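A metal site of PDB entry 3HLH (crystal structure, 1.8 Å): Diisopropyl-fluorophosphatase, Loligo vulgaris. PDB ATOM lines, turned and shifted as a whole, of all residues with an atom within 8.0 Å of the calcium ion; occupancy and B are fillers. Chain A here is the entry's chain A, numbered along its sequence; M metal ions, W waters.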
ATOM      1  N   GLU A  21      -7.148  23.690  -4.389  1.00  0.00           N
ATOM      2  CA  GLU A  21      -5.883  24.366  -4.640  1.00  0.00           C
ATOM      3  C   GLU A  21      -4.794  23.431  -5.139  1.00  0.00           C
ATOM      4  O   GLU A  21      -5.047  22.248  -5.416  1.00  0.00           O
ATOM      5  CB  GLU A  21      -5.407  25.037  -3.346  1.00  0.00           C
ATOM      6  CG  GLU A  21      -5.531  26.551  -3.339  1.00  0.00           C
ATOM      7  CD  GLU A  21      -4.309  27.243  -3.936  1.00  0.00           C
ATOM      8  OE1 GLU A  21      -3.564  26.601  -4.704  1.00  0.00           O
ATOM      9  OE2 GLU A  21      -4.107  28.433  -3.630  1.00  0.00           O
ATOM     10  N   GLY A  22      -3.587  23.973  -5.268  1.00  0.00           N
ATOM     11  CA  GLY A  22      -2.420  23.214  -5.693  1.00  0.00           C
ATOM     12  C   GLY A  22      -2.533  22.263  -6.879  1.00  0.00           C
ATOM     13  O   GLY A  22      -2.096  21.114  -6.773  1.00  0.00           O
ATOM     14  N   PRO A  23      -3.098  22.702  -8.008  1.00  0.00           N
ATOM     15  CA  PRO A  23      -3.195  21.792  -9.153  1.00  0.00           C
ATOM     16  C   PRO A  23      -1.792  21.445  -9.644  1.00  0.00           C
ATOM     17  O   PRO A  23      -0.934  22.322  -9.752  1.00  0.00           O
ATOM     18  CB  PRO A  23      -3.986  22.600 -10.168  1.00  0.00           C
ATOM     19  CG  PRO A  23      -3.563  24.013  -9.864  1.00  0.00           C
ATOM     20  CD  PRO A  23      -3.614  24.037  -8.363  1.00  0.00           C
ATOM     21  N   VAL A  24      -1.561  20.174  -9.950  1.00  0.00           N
ATOM     22  CA  VAL A  24      -0.240  19.766 -10.413  1.00  0.00           C
ATOM     23  C   VAL A  24      -0.294  18.444 -11.161  1.00  0.00           C
ATOM     24  O   VAL A  24      -1.195  17.634 -10.957  1.00  0.00           O
ATOM     25  CB  VAL A  24       0.746  19.658  -9.224  1.00  0.00           C
ATOM     26  CG1 VAL A  24       0.306  18.530  -8.278  1.00  0.00           C
ATOM     27  CG2 VAL A  24       2.161  19.432  -9.728  1.00  0.00           C
ATOM     28  N   PHE A  25       0.685  18.246 -12.035  1.00  0.00           N
ATOM     29  CA  PHE A  25       0.820  17.008 -12.807  1.00  0.00           C
ATOM     30  C   PHE A  25       2.135  16.380 -12.376  1.00  0.00           C
ATOM     31  O   PHE A  25       3.111  17.092 -12.136  1.00  0.00           O
ATOM     32  CB  PHE A  25       0.888  17.318 -14.309  1.00  0.00           C
ATOM     33  CG  PHE A  25      -0.438  17.595 -14.942  1.00  0.00           C
ATOM     34  CD1 PHE A  25      -1.315  16.559 -15.256  1.00  0.00           C
ATOM     35  CD2 PHE A  25      -0.829  18.912 -15.209  1.00  0.00           C
ATOM     36  CE1 PHE A  25      -2.546  16.811 -15.841  1.00  0.00           C
ATOM     37  CE2 PHE A  25      -2.068  19.177 -15.787  1.00  0.00           C
ATOM     38  CZ  PHE A  25      -2.926  18.126 -16.108  1.00  0.00           C
ATOM     39  N   CYS A  76       1.430  22.699  -4.477  1.00  0.00           N
ATOM     40  CA  CYS A  76       2.234  21.544  -4.892  1.00  0.00           C
ATOM     41  C   CYS A  76       3.213  21.809  -6.032  1.00  0.00           C
ATOM     42  O   CYS A  76       3.052  22.731  -6.833  1.00  0.00           O
ATOM     43  CB  CYS A  76       1.326  20.406  -5.364  1.00  0.00           C
ATOM     44  SG  CYS A  76      -0.004  19.920  -4.263  1.00  0.00           S
ATOM     45  N   GLN A  77       4.237  20.959  -6.088  1.00  0.00           N
ATOM     46  CA  GLN A  77       5.235  21.005  -7.135  1.00  0.00           C
ATOM     47  C   GLN A  77       5.656  19.560  -7.372  1.00  0.00           C
ATOM     48  O   GLN A  77       5.794  18.777  -6.434  1.00  0.00           O
ATOM     49  CB  GLN A  77       6.457  21.833  -6.732  1.00  0.00           C
ATOM     50  CG  GLN A  77       6.313  23.352  -6.944  1.00  0.00           C
ATOM     51  CD  GLN A  77       6.055  23.724  -8.399  1.00  0.00           C
ATOM     52  OE1 GLN A  77       4.921  23.682  -8.880  1.00  0.00           O
ATOM     53  NE2 GLN A  77       7.113  24.089  -9.101  1.00  0.00           N
ATOM     54  N   ASP A 121       2.356  27.985  -1.033  1.00  0.00           N
ATOM     55  CA  ASP A 121       2.660  27.521  -2.390  1.00  0.00           C
ATOM     56  C   ASP A 121       4.176  27.435  -2.560  1.00  0.00           C
ATOM     57  O   ASP A 121       4.937  27.932  -1.728  1.00  0.00           O
ATOM     58  CB  ASP A 121       2.058  28.475  -3.437  1.00  0.00           C
ATOM     59  CG  ASP A 121       1.690  27.781  -4.745  1.00  0.00           C
ATOM     60  OD1 ASP A 121       1.998  26.580  -4.905  1.00  0.00           O
ATOM     61  OD2 ASP A 121       1.069  28.428  -5.621  1.00  0.00           O
ATOM     62  N   CYS A 122       4.612  26.803  -3.641  1.00  0.00           N
ATOM     63  CA  CYS A 122       6.030  26.657  -3.899  1.00  0.00           C
ATOM     64  C   CYS A 122       6.315  26.516  -5.398  1.00  0.00           C
ATOM     65  O   CYS A 122       5.418  26.187  -6.173  1.00  0.00           O
ATOM     66  CB  CYS A 122       6.601  25.449  -3.133  1.00  0.00           C
ATOM     67  SG  CYS A 122       5.801  23.858  -3.457  1.00  0.00           S
ATOM     68  N   ILE A 177       3.921  32.164  -6.146  1.00  0.00           N
ATOM     69  CA  ILE A 177       5.352  32.338  -6.348  1.00  0.00           C
ATOM     70  C   ILE A 177       5.762  31.675  -7.669  1.00  0.00           C
ATOM     71  O   ILE A 177       5.144  30.694  -8.105  1.00  0.00           O
ATOM     72  CB  ILE A 177       6.137  31.721  -5.148  1.00  0.00           C
ATOM     73  CG1 ILE A 177       7.618  32.098  -5.232  1.00  0.00           C
ATOM     74  CG2 ILE A 177       5.946  30.211  -5.124  1.00  0.00           C
ATOM     75  CD1 ILE A 177       8.376  31.873  -3.935  1.00  0.00           C
ATOM     76  N   GLY A 230      -2.338  31.984  -6.809  1.00  0.00           N
ATOM     77  CA  GLY A 230      -1.366  31.188  -7.566  1.00  0.00           C
ATOM     78  C   GLY A 230      -0.934  31.761  -8.905  1.00  0.00           C
ATOM     79  O   GLY A 230      -1.659  32.520  -9.532  1.00  0.00           O
ATOM     80  N   MET A 231       0.257  31.371  -9.352  1.00  0.00           N
ATOM     81  CA  MET A 231       0.803  31.863 -10.607  1.00  0.00           C
ATOM     82  C   MET A 231       1.668  30.854 -11.364  1.00  0.00           C
ATOM     83  O   MET A 231       2.133  29.875 -10.788  1.00  0.00           O
ATOM     84  CB  MET A 231       1.638  33.115 -10.342  1.00  0.00           C
ATOM     85  CG  MET A 231       2.775  32.891  -9.349  1.00  0.00           C
ATOM     86  SD  MET A 231       3.811  34.365  -9.097  1.00  0.00           S
ATOM     87  CE  MET A 231       2.562  35.550  -8.606  1.00  0.00           C
ATOM     88  N   ASP A 232       1.861  31.116 -12.656  1.00  0.00           N
ATOM     89  CA  ASP A 232       2.697  30.273 -13.513  1.00  0.00           C
ATOM     90  C   ASP A 232       2.995  31.022 -14.808  1.00  0.00           C
ATOM     91  O   ASP A 232       2.215  31.864 -15.250  1.00  0.00           O
ATOM     92  CB  ASP A 232       1.996  28.952 -13.862  1.00  0.00           C
ATOM     93  CG  ASP A 232       2.379  27.816 -12.929  1.00  0.00           C
ATOM     94  OD1 ASP A 232       3.562  27.710 -12.531  1.00  0.00           O
ATOM     95  OD2 ASP A 232       1.483  27.009 -12.601  1.00  0.00           O
ATOM     96  N   PHE A 233       4.134  30.703 -15.410  1.00  0.00           N
ATOM     97  CA  PHE A 233       4.560  31.322 -16.668  1.00  0.00           C
ATOM     98  C   PHE A 233       4.112  30.484 -17.863  1.00  0.00           C
ATOM     99  O   PHE A 233       4.007  29.257 -17.753  1.00  0.00           O
ATOM    100  CB  PHE A 233       6.086  31.382 -16.725  1.00  0.00           C
ATOM    101  CG  PHE A 233       6.705  32.466 -15.892  1.00  0.00           C
ATOM    102  CD1 PHE A 233       6.607  33.799 -16.280  1.00  0.00           C
ATOM    103  CD2 PHE A 233       7.402  32.148 -14.735  1.00  0.00           C
ATOM    104  CE1 PHE A 233       7.196  34.811 -15.531  1.00  0.00           C
ATOM    105  CE2 PHE A 233       7.999  33.155 -13.964  1.00  0.00           C
ATOM    106  CZ  PHE A 233       7.901  34.483 -14.371  1.00  0.00           C
ATOM    107  N   LEU A 240       0.885  34.342 -15.686  1.00  0.00           N
ATOM    108  CA  LEU A 240      -0.561  34.260 -15.468  1.00  0.00           C
ATOM    109  C   LEU A 240      -0.785  34.167 -13.975  1.00  0.00           C
ATOM    110  O   LEU A 240      -0.247  33.274 -13.309  1.00  0.00           O
ATOM    111  CB  LEU A 240      -1.156  33.048 -16.181  1.00  0.00           C
ATOM    112  CG  LEU A 240      -1.276  33.143 -17.704  1.00  0.00           C
ATOM    113  CD1 LEU A 240       0.113  33.085 -18.340  1.00  0.00           C
ATOM    114  CD2 LEU A 240      -2.139  32.013 -18.231  1.00  0.00           C
ATOM    115  N   ASN A 272      -5.790  29.032  -8.074  1.00  0.00           N
ATOM    116  CA  ASN A 272      -4.525  28.621  -8.660  1.00  0.00           C
ATOM    117  C   ASN A 272      -4.712  28.064 -10.071  1.00  0.00           C
ATOM    118  O   ASN A 272      -5.836  27.906 -10.540  1.00  0.00           O
ATOM    119  CB  ASN A 272      -3.862  27.567  -7.773  1.00  0.00           C
ATOM    120  CG  ASN A 272      -2.364  27.738  -7.684  1.00  0.00           C
ATOM    121  OD1 ASN A 272      -1.706  28.063  -8.673  1.00  0.00           O
ATOM    122  ND2 ASN A 272      -1.815  27.508  -6.499  1.00  0.00           N
ATOM    123  N   LEU A 273      -3.599  27.755 -10.727  1.00  0.00           N
ATOM    124  CA  LEU A 273      -3.653  27.224 -12.073  1.00  0.00           C
ATOM    125  C   LEU A 273      -2.412  26.391 -12.374  1.00  0.00           C
ATOM    126  O   LEU A 273      -1.398  26.495 -11.681  1.00  0.00           O
ATOM    127  CB  LEU A 273      -3.798  28.358 -13.080  1.00  0.00           C
ATOM    128  CG  LEU A 273      -2.731  29.461 -13.149  1.00  0.00           C
ATOM    129  CD1 LEU A 273      -1.497  28.952 -13.874  1.00  0.00           C
ATOM    130  CD2 LEU A 273      -3.295  30.648 -13.909  1.00  0.00           C
ATOM    131  N   HIS A 274      -2.500  25.564 -13.407  1.00  0.00           N
ATOM    132  CA  HIS A 274      -1.378  24.727 -13.799  1.00  0.00           C
ATOM    133  C   HIS A 274      -1.605  24.284 -15.242  1.00  0.00           C
ATOM    134  O   HIS A 274      -2.728  23.925 -15.602  1.00  0.00           O
ATOM    135  CB  HIS A 274      -1.273  23.508 -12.893  1.00  0.00           C
ATOM    136  CG  HIS A 274       0.137  23.017 -12.699  1.00  0.00           C
ATOM    137  ND1 HIS A 274       1.086  23.745 -12.006  1.00  0.00           N
ATOM    138  CD2 HIS A 274       0.752  21.888 -13.110  1.00  0.00           C
ATOM    139  CE1 HIS A 274       2.221  23.082 -12.001  1.00  0.00           C
ATOM    140  NE2 HIS A 274       2.053  21.943 -12.664  1.00  0.00           N
ATOM    141  N   PHE A 275      -0.559  24.313 -16.056  1.00  0.00           N
ATOM    142  CA  PHE A 275      -0.672  23.894 -17.454  1.00  0.00           C
ATOM    143  C   PHE A 275      -0.541  22.390 -17.569  1.00  0.00           C
ATOM    144  O   PHE A 275       0.117  21.764 -16.740  1.00  0.00           O
ATOM    145  CB  PHE A 275       0.453  24.489 -18.305  1.00  0.00           C
ATOM    146  CG  PHE A 275       0.251  25.918 -18.720  1.00  0.00           C
ATOM    147  CD1 PHE A 275       0.545  26.956 -17.851  1.00  0.00           C
ATOM    148  CD2 PHE A 275      -0.209  26.218 -20.008  1.00  0.00           C
ATOM    149  CE1 PHE A 275       0.418  28.289 -18.260  1.00  0.00           C
ATOM    150  CE2 PHE A 275      -0.349  27.540 -20.424  1.00  0.00           C
ATOM    151  CZ  PHE A 275      -0.035  28.577 -19.545  1.00  0.00           C
ATOM    152  N   ILE A 282      -5.066  24.925 -19.511  1.00  0.00           N
ATOM    153  CA  ILE A 282      -4.782  25.382 -18.166  1.00  0.00           C
ATOM    154  C   ILE A 282      -5.889  24.912 -17.237  1.00  0.00           C
ATOM    155  O   ILE A 282      -7.065  25.151 -17.496  1.00  0.00           O
ATOM    156  CB  ILE A 282      -4.713  26.920 -18.062  1.00  0.00           C
ATOM    157  CG1 ILE A 282      -3.577  27.456 -18.927  1.00  0.00           C
ATOM    158  CG2 ILE A 282      -4.533  27.334 -16.601  1.00  0.00           C
ATOM    159  CD1 ILE A 282      -3.496  28.972 -18.963  1.00  0.00           C
ATOM    160  N   PHE A 283      -5.506  24.228 -16.161  1.00  0.00           N
ATOM    161  CA  PHE A 283      -6.479  23.778 -15.187  1.00  0.00           C
ATOM    162  C   PHE A 283      -6.507  24.833 -14.093  1.00  0.00           C
ATOM    163  O   PHE A 283      -5.461  25.297 -13.638  1.00  0.00           O
ATOM    164  CB  PHE A 283      -6.110  22.409 -14.634  1.00  0.00           C
ATOM    165  CG  PHE A 283      -6.349  21.307 -15.620  1.00  0.00           C
ATOM    166  CD1 PHE A 283      -5.508  21.137 -16.709  1.00  0.00           C
ATOM    167  CD2 PHE A 283      -7.472  20.484 -15.494  1.00  0.00           C
ATOM    168  CE1 PHE A 283      -5.787  20.162 -17.678  1.00  0.00           C
ATOM    169  CE2 PHE A 283      -7.760  19.514 -16.455  1.00  0.00           C
ATOM    170  CZ  PHE A 283      -6.908  19.352 -17.546  1.00  0.00           C
ATOM    171  N   GLN A 304       7.666  22.819 -16.321  1.00  0.00           N
ATOM    172  CA  GLN A 304       7.857  22.760 -14.882  1.00  0.00           C
ATOM    173  C   GLN A 304       9.157  21.988 -14.670  1.00  0.00           C
ATOM    174  O   GLN A 304       9.625  21.297 -15.568  1.00  0.00           O
ATOM    175  CB  GLN A 304       6.705  22.030 -14.190  1.00  0.00           C
ATOM    176  CG  GLN A 304       5.418  22.836 -14.090  1.00  0.00           C
ATOM    177  CD  GLN A 304       5.489  23.927 -13.027  1.00  0.00           C
ATOM    178  OE1 GLN A 304       5.536  25.117 -13.344  1.00  0.00           O
ATOM    179  NE2 GLN A 304       5.505  23.512 -11.766  1.00  0.00           N
HETATM  180 CA    CA M   1       0.728  25.883 -10.927  1.00  0.00          CA
HETATM  181  O   HOH W   1       3.020  25.766 -10.365  1.00  0.00           O
HETATM  182  O   HOH W   2      -0.265  24.762  -9.127  1.00  0.00           O
HETATM  183  O   HOH W   3       0.711  27.895  -9.543  1.00  0.00           O
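The calcium ion is bound by the side-chain carboxylate (OD2) of Asp 232 (2.2 Å), the backbone carbonyl oxygen (O) of Leu 273 (2.3 Å), water W2 (2.3 Å), water W1 (2.4 Å), a ring nitrogen (ND1) of His 274 (2.4 Å) and water W3 (2.4 Å).
The calcium ion has six donor atoms within binding distance.
Merely in contact with the calcium ion: Asn 272.
Of the 22 residues printed, 4 come within 4 Å of the calcium ion.
Water W3 lies within hydrogen-bond range of the side-chain amide oxygen (OD1) of Asn 272 and the backbone carbonyl oxygen (O) of Met 231.
Water W1 lies within hydrogen-bond range of the side-chain carboxylate (OD1) of Asp 232 and the side-chain amide oxygen (OE1) of Gln 77.
The side-chain carboxylate (OD1) of Asp 232 sits close to the side-chain amide oxygen (OE1) of Gln 304 (3.4 Å).
N of Leu 240 is in hydrogen-bond range of O of Asp 232.
The backbone carbonyl oxygen (O) of Pro 23 sits close to a ring nitrogen (ND1) of His 274, at 3.3 Å.
N of Phe 283 sits at hydrogen-bond distance from O of His 274 (2.8 Å).
OD2 of Asp 121 sits at hydrogen-bond distance from ND2 of Asn 272 (3.2 Å).
The side-chain amide nitrogen of Asn 272 is in hydrogen-bond range of the side-chain carboxylate of Glu 21 (2.7 Å).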
